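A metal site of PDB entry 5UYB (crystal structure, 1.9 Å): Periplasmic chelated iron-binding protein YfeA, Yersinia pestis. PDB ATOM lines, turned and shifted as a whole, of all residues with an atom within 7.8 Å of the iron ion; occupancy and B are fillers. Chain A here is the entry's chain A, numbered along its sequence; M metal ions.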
ATOM      1  N   GLU A  74       5.311   8.326  23.336  1.00  0.00           N
ATOM      2  CA  GLU A  74       5.053   9.494  22.497  1.00  0.00           C
ATOM      3  C   GLU A  74       3.615   9.420  21.959  1.00  0.00           C
ATOM      4  O   GLU A  74       3.251   8.434  21.326  1.00  0.00           O
ATOM      5  CB  GLU A  74       6.082   9.523  21.368  1.00  0.00           C
ATOM      6  CG  GLU A  74       6.291  10.890  20.759  1.00  0.00           C
ATOM      7  CD  GLU A  74       5.069  11.350  20.008  1.00  0.00           C
ATOM      8  OE1 GLU A  74       4.658  10.638  19.047  1.00  0.00           O
ATOM      9  OE2 GLU A  74       4.500  12.394  20.389  1.00  0.00           O
ATOM     10  N   ILE A  75       2.829  10.466  22.198  1.00  0.00           N
ATOM     11  CA  ILE A  75       1.378  10.409  21.978  1.00  0.00           C
ATOM     12  C   ILE A  75       0.912  10.940  20.626  1.00  0.00           C
ATOM     13  O   ILE A  75      -0.185  10.568  20.170  1.00  0.00           O
ATOM     14  CB  ILE A  75       0.643  11.175  23.103  1.00  0.00           C
ATOM     15  CG1 ILE A  75       0.954  12.682  23.014  1.00  0.00           C
ATOM     16  CG2 ILE A  75       1.062  10.632  24.447  1.00  0.00           C
ATOM     17  CD1 ILE A  75       0.259  13.532  24.087  1.00  0.00           C
ATOM     18  N   HIS A  76       1.687  11.814  19.973  1.00  0.00           N
ATOM     19  CA  HIS A  76       1.221  12.442  18.729  1.00  0.00           C
ATOM     20  C   HIS A  76       1.144  11.419  17.602  1.00  0.00           C
ATOM     21  O   HIS A  76       0.143  11.346  16.867  1.00  0.00           O
ATOM     22  CB  HIS A  76       2.158  13.585  18.347  1.00  0.00           C
ATOM     23  CG  HIS A  76       2.160  14.733  19.302  1.00  0.00           C
ATOM     24  ND1 HIS A  76       1.554  15.940  19.016  1.00  0.00           N
ATOM     25  CD2 HIS A  76       2.728  14.883  20.534  1.00  0.00           C
ATOM     26  CE1 HIS A  76       1.746  16.785  20.027  1.00  0.00           C
ATOM     27  NE2 HIS A  76       2.461  16.160  20.951  1.00  0.00           N
ATOM     28  N   LEU A 101      -4.172  16.583  18.313  1.00  0.00           N
ATOM     29  CA  LEU A 101      -3.169  15.913  19.128  1.00  0.00           C
ATOM     30  C   LEU A 101      -2.936  14.501  18.610  1.00  0.00           C
ATOM     31  O   LEU A 101      -1.841  14.172  18.137  1.00  0.00           O
ATOM     32  CB  LEU A 101      -3.590  15.896  20.611  1.00  0.00           C
ATOM     33  CG  LEU A 101      -2.622  15.138  21.524  1.00  0.00           C
ATOM     34  CD1 LEU A 101      -1.259  15.841  21.623  1.00  0.00           C
ATOM     35  CD2 LEU A 101      -3.217  14.959  22.901  1.00  0.00           C
ATOM     36  N   ASN A 139      -2.712  24.427  18.216  1.00  0.00           N
ATOM     37  CA  ASN A 139      -1.732  23.767  19.097  1.00  0.00           C
ATOM     38  C   ASN A 139      -2.504  22.881  20.071  1.00  0.00           C
ATOM     39  O   ASN A 139      -3.380  23.391  20.784  1.00  0.00           O
ATOM     40  CB  ASN A 139      -0.903  24.834  19.828  1.00  0.00           C
ATOM     41  CG  ASN A 139       0.231  24.267  20.650  1.00  0.00           C
ATOM     42  OD1 ASN A 139       0.111  23.205  21.271  1.00  0.00           O
ATOM     43  ND2 ASN A 139       1.339  24.987  20.690  1.00  0.00           N
ATOM     44  N   PRO A 140      -2.235  21.573  20.146  1.00  0.00           N
ATOM     45  CA  PRO A 140      -3.073  20.699  20.991  1.00  0.00           C
ATOM     46  C   PRO A 140      -2.834  20.829  22.486  1.00  0.00           C
ATOM     47  O   PRO A 140      -3.708  20.402  23.261  1.00  0.00           O
ATOM     48  CB  PRO A 140      -2.689  19.286  20.510  1.00  0.00           C
ATOM     49  CG  PRO A 140      -1.267  19.424  20.073  1.00  0.00           C
ATOM     50  CD  PRO A 140      -1.224  20.796  19.388  1.00  0.00           C
ATOM     51  N   HIS A 141      -1.727  21.417  22.933  1.00  0.00           N
ATOM     52  CA  HIS A 141      -1.312  21.241  24.320  1.00  0.00           C
ATOM     53  C   HIS A 141      -2.041  22.180  25.276  1.00  0.00           C
ATOM     54  O   HIS A 141      -1.411  22.770  26.160  1.00  0.00           O
ATOM     55  CB  HIS A 141       0.200  21.441  24.461  1.00  0.00           C
ATOM     56  CG  HIS A 141       1.005  20.545  23.552  1.00  0.00           C
ATOM     57  ND1 HIS A 141       1.358  20.917  22.275  1.00  0.00           N
ATOM     58  CD2 HIS A 141       1.481  19.295  23.734  1.00  0.00           C
ATOM     59  CE1 HIS A 141       2.035  19.930  21.715  1.00  0.00           C
ATOM     60  NE2 HIS A 141       2.131  18.937  22.573  1.00  0.00           N
ATOM     61  N   TRP A 143      -3.962  21.710  27.834  1.00  0.00           N
ATOM     62  CA  TRP A 143      -3.988  21.356  29.251  1.00  0.00           C
ATOM     63  C   TRP A 143      -2.858  21.988  30.070  1.00  0.00           C
ATOM     64  O   TRP A 143      -2.902  21.909  31.308  1.00  0.00           O
ATOM     65  CB  TRP A 143      -3.944  19.821  29.383  1.00  0.00           C
ATOM     66  CG  TRP A 143      -2.669  19.213  28.870  1.00  0.00           C
ATOM     67  CD1 TRP A 143      -1.506  19.078  29.556  1.00  0.00           C
ATOM     68  CD2 TRP A 143      -2.438  18.656  27.567  1.00  0.00           C
ATOM     69  NE1 TRP A 143      -0.554  18.484  28.761  1.00  0.00           N
ATOM     70  CE2 TRP A 143      -1.114  18.215  27.529  1.00  0.00           C
ATOM     71  CE3 TRP A 143      -3.227  18.502  26.423  1.00  0.00           C
ATOM     72  CZ2 TRP A 143      -0.543  17.606  26.405  1.00  0.00           C
ATOM     73  CZ3 TRP A 143      -2.681  17.909  25.298  1.00  0.00           C
ATOM     74  CH2 TRP A 143      -1.342  17.464  25.298  1.00  0.00           C
ATOM     75  N   GLU A 207      10.065  20.445  22.000  1.00  0.00           N
ATOM     76  CA  GLU A 207       8.788  20.652  21.326  1.00  0.00           C
ATOM     77  C   GLU A 207       8.198  21.980  21.796  1.00  0.00           C
ATOM     78  O   GLU A 207       8.324  22.353  22.970  1.00  0.00           O
ATOM     79  CB  GLU A 207       7.798  19.500  21.599  1.00  0.00           C
ATOM     80  CG  GLU A 207       6.425  19.684  20.909  1.00  0.00           C
ATOM     81  CD  GLU A 207       5.400  18.571  21.214  1.00  0.00           C
ATOM     82  OE1 GLU A 207       5.359  18.007  22.332  1.00  0.00           O
ATOM     83  OE2 GLU A 207       4.611  18.267  20.298  1.00  0.00           O
ATOM     84  N   GLY A 208       7.546  22.685  20.882  1.00  0.00           N
ATOM     85  CA  GLY A 208       6.815  23.897  21.239  1.00  0.00           C
ATOM     86  C   GLY A 208       5.492  23.549  21.896  1.00  0.00           C
ATOM     87  O   GLY A 208       4.430  23.970  21.438  1.00  0.00           O
ATOM     88  N   ALA A 209       5.559  22.783  22.981  1.00  0.00           N
ATOM     89  CA  ALA A 209       4.383  22.249  23.653  1.00  0.00           C
ATOM     90  C   ALA A 209       3.867  23.157  24.760  1.00  0.00           C
ATOM     91  O   ALA A 209       2.878  22.812  25.412  1.00  0.00           O
ATOM     92  CB  ALA A 209       4.689  20.873  24.252  1.00  0.00           C
ATOM     93  N   PHE A 210       4.508  24.296  24.994  1.00  0.00           N
ATOM     94  CA  PHE A 210       4.216  25.083  26.189  1.00  0.00           C
ATOM     95  C   PHE A 210       3.544  26.415  25.864  1.00  0.00           C
ATOM     96  O   PHE A 210       3.471  27.287  26.735  1.00  0.00           O
ATOM     97  CB  PHE A 210       5.500  25.270  26.997  1.00  0.00           C
ATOM     98  CG  PHE A 210       6.110  23.955  27.421  1.00  0.00           C
ATOM     99  CD1 PHE A 210       5.676  23.319  28.564  1.00  0.00           C
ATOM    100  CD2 PHE A 210       7.060  23.334  26.613  1.00  0.00           C
ATOM    101  CE1 PHE A 210       6.216  22.063  28.949  1.00  0.00           C
ATOM    102  CE2 PHE A 210       7.588  22.091  26.980  1.00  0.00           C
ATOM    103  CZ  PHE A 210       7.171  21.457  28.149  1.00  0.00           C
ATOM    104  N   TRP A 225      11.399  22.304  17.723  1.00  0.00           N
ATOM    105  CA  TRP A 225      10.432  21.954  16.691  1.00  0.00           C
ATOM    106  C   TRP A 225       9.040  22.335  17.180  1.00  0.00           C
ATOM    107  O   TRP A 225       8.774  22.289  18.384  1.00  0.00           O
ATOM    108  CB  TRP A 225      10.484  20.466  16.308  1.00  0.00           C
ATOM    109  CG  TRP A 225      10.371  19.469  17.441  1.00  0.00           C
ATOM    110  CD1 TRP A 225       9.221  18.880  17.911  1.00  0.00           C
ATOM    111  CD2 TRP A 225      11.449  18.910  18.202  1.00  0.00           C
ATOM    112  NE1 TRP A 225       9.535  17.994  18.937  1.00  0.00           N
ATOM    113  CE2 TRP A 225      10.887  18.003  19.138  1.00  0.00           C
ATOM    114  CE3 TRP A 225      12.833  19.094  18.197  1.00  0.00           C
ATOM    115  CZ2 TRP A 225      11.668  17.286  20.045  1.00  0.00           C
ATOM    116  CZ3 TRP A 225      13.613  18.386  19.101  1.00  0.00           C
ATOM    117  CH2 TRP A 225      13.020  17.487  20.015  1.00  0.00           C
ATOM    118  N   PRO A 226       8.145  22.749  16.276  1.00  0.00           N
ATOM    119  CA  PRO A 226       6.845  23.286  16.733  1.00  0.00           C
ATOM    120  C   PRO A 226       5.908  22.223  17.315  1.00  0.00           C
ATOM    121  O   PRO A 226       5.172  22.522  18.257  1.00  0.00           O
ATOM    122  CB  PRO A 226       6.253  23.929  15.473  1.00  0.00           C
ATOM    123  CG  PRO A 226       6.997  23.301  14.334  1.00  0.00           C
ATOM    124  CD  PRO A 226       8.364  22.965  14.837  1.00  0.00           C
ATOM    125  N   ILE A 227       5.928  21.002  16.795  1.00  0.00           N
ATOM    126  CA  ILE A 227       5.070  19.930  17.291  1.00  0.00           C
ATOM    127  C   ILE A 227       5.719  18.618  16.884  1.00  0.00           C
ATOM    128  O   ILE A 227       6.343  18.513  15.822  1.00  0.00           O
ATOM    129  CB  ILE A 227       3.622  20.063  16.753  1.00  0.00           C
ATOM    130  CG1 ILE A 227       2.692  19.001  17.358  1.00  0.00           C
ATOM    131  CG2 ILE A 227       3.580  19.995  15.240  1.00  0.00           C
ATOM    132  CD1 ILE A 227       1.204  19.336  17.153  1.00  0.00           C
ATOM    133  N   ASN A 228       5.624  17.623  17.770  1.00  0.00           N
ATOM    134  CA  ASN A 228       6.208  16.319  17.497  1.00  0.00           C
ATOM    135  C   ASN A 228       5.726  15.817  16.138  1.00  0.00           C
ATOM    136  O   ASN A 228       4.533  15.862  15.837  1.00  0.00           O
ATOM    137  CB  ASN A 228       5.845  15.333  18.608  1.00  0.00           C
ATOM    138  CG  ASN A 228       6.550  15.637  19.917  1.00  0.00           C
ATOM    139  OD1 ASN A 228       7.366  16.542  20.005  1.00  0.00           O
ATOM    140  ND2 ASN A 228       6.233  14.855  20.946  1.00  0.00           N
ATOM    141  N   GLU A 256      11.694  17.476  27.125  1.00  0.00           N
ATOM    142  CA  GLU A 256      10.445  16.943  27.669  1.00  0.00           C
ATOM    143  C   GLU A 256      10.506  15.428  27.733  1.00  0.00           C
ATOM    144  O   GLU A 256      11.322  14.787  27.074  1.00  0.00           O
ATOM    145  CB  GLU A 256       9.241  17.382  26.832  1.00  0.00           C
ATOM    146  CG  GLU A 256       9.144  18.896  26.673  1.00  0.00           C
ATOM    147  CD  GLU A 256       9.944  19.385  25.487  1.00  0.00           C
ATOM    148  OE1 GLU A 256       9.772  18.813  24.383  1.00  0.00           O
ATOM    149  OE2 GLU A 256      10.759  20.330  25.647  1.00  0.00           O
ATOM    150  N   THR A 258       8.821  12.676  26.867  1.00  0.00           N
ATOM    151  CA  THR A 258       8.583  11.616  25.888  1.00  0.00           C
ATOM    152  C   THR A 258       9.481  11.690  24.657  1.00  0.00           C
ATOM    153  O   THR A 258       9.338  10.867  23.759  1.00  0.00           O
ATOM    154  CB  THR A 258       7.123  11.588  25.416  1.00  0.00           C
ATOM    155  OG1 THR A 258       6.850  12.733  24.580  1.00  0.00           O
ATOM    156  CG2 THR A 258       6.159  11.557  26.593  1.00  0.00           C
ATOM    157  N   ILE A 259      10.389  12.660  24.591  1.00  0.00           N
ATOM    158  CA  ILE A 259      11.261  12.836  23.437  1.00  0.00           C
ATOM    159  C   ILE A 259      12.714  12.807  23.906  1.00  0.00           C
ATOM    160  O   ILE A 259      13.006  12.750  25.100  1.00  0.00           O
ATOM    161  CB  ILE A 259      10.933  14.124  22.657  1.00  0.00           C
ATOM    162  CG1 ILE A 259      10.801  15.312  23.607  1.00  0.00           C
ATOM    163  CG2 ILE A 259       9.640  13.966  21.869  1.00  0.00           C
ATOM    164  CD1 ILE A 259      12.128  16.040  23.895  1.00  0.00           C
ATOM    165  N   VAL A 281       4.843  17.308  29.866  1.00  0.00           N
ATOM    166  CA  VAL A 281       3.706  17.898  29.155  1.00  0.00           C
ATOM    167  C   VAL A 281       2.873  16.811  28.485  1.00  0.00           C
ATOM    168  O   VAL A 281       1.646  16.754  28.681  1.00  0.00           O
ATOM    169  CB  VAL A 281       4.170  18.962  28.139  1.00  0.00           C
ATOM    170  CG1 VAL A 281       5.328  18.465  27.274  1.00  0.00           C
ATOM    171  CG2 VAL A 281       2.976  19.425  27.274  1.00  0.00           C
ATOM    172  N   ASP A 282       3.504  15.937  27.710  1.00  0.00           N
ATOM    173  CA  ASP A 282       2.765  14.963  26.925  1.00  0.00           C
ATOM    174  C   ASP A 282       2.428  13.700  27.716  1.00  0.00           C
ATOM    175  O   ASP A 282       1.579  12.916  27.262  1.00  0.00           O
ATOM    176  CB  ASP A 282       3.552  14.573  25.679  1.00  0.00           C
ATOM    177  CG  ASP A 282       3.453  15.616  24.563  1.00  0.00           C
ATOM    178  OD1 ASP A 282       2.790  16.655  24.759  1.00  0.00           O
ATOM    179  OD2 ASP A 282       4.039  15.377  23.486  1.00  0.00           O
ATOM    180  N   SER A 283       3.049  13.477  28.866  1.00  0.00           N
ATOM    181  CA  SER A 283       2.774  12.249  29.606  1.00  0.00           C
ATOM    182  C   SER A 283       3.040  12.488  31.091  1.00  0.00           C
ATOM    183  O   SER A 283       3.942  13.239  31.462  1.00  0.00           O
ATOM    184  CB  SER A 283       3.625  11.081  29.088  1.00  0.00           C
ATOM    185  OG  SER A 283       3.399   9.886  29.861  1.00  0.00           O
HETATM  186 FE    FE M   1       3.452  17.177  22.437  1.00  0.00          FE
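OE2 of Glu 74 lies within hydrogen-bond range of N of His 76 (2.9 Å). N of Asn 228 lies within hydrogen-bond range of OE2 of Glu 207, 2.8 Å away. OE1 of Glu 256 sits at hydrogen-bond distance from N of Glu 207 (2.9 Å). The side-chain amide nitrogen (ND2) of Asn 228 sits close to the side-chain carboxylate (OD2) of Asp 282. The side-chain amide oxygen of Asn 139 sits at hydrogen-bond distance from a ring nitrogen (ND1) of His 141 (2.8 Å). The side-chain amide nitrogen (ND2) of Asn 228 sits at hydrogen-bond distance from the side-chain carboxylate (OE2) of Glu 74, at 3.1 Å. NE1 of Trp 225 lies within hydrogen-bond range of OD1 of Asn 228, at 2.8 Å.
Merely in contact with the iron ion: Asn 228. Five residues have an atom within 4 Å of the iron ion: His 76, His 141, Glu 207, Asn 228 and Asp 282. The nearest printed residue that does not touch the iron ion is Ala 209 (4.3 Å).
The iron ion is bound by NE2 of His 76 (2.1 Å), OE1 of Glu 207 (2.1 Å), OD2 of Asp 282 (2.2 Å), NE2 of His 141 (2.2 Å) and OD1 of Asp 282 (2.5 Å). Slightly farther from the iron ion lies the side-chain carboxylate (OE2) of Glu 207 (2.7 Å).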
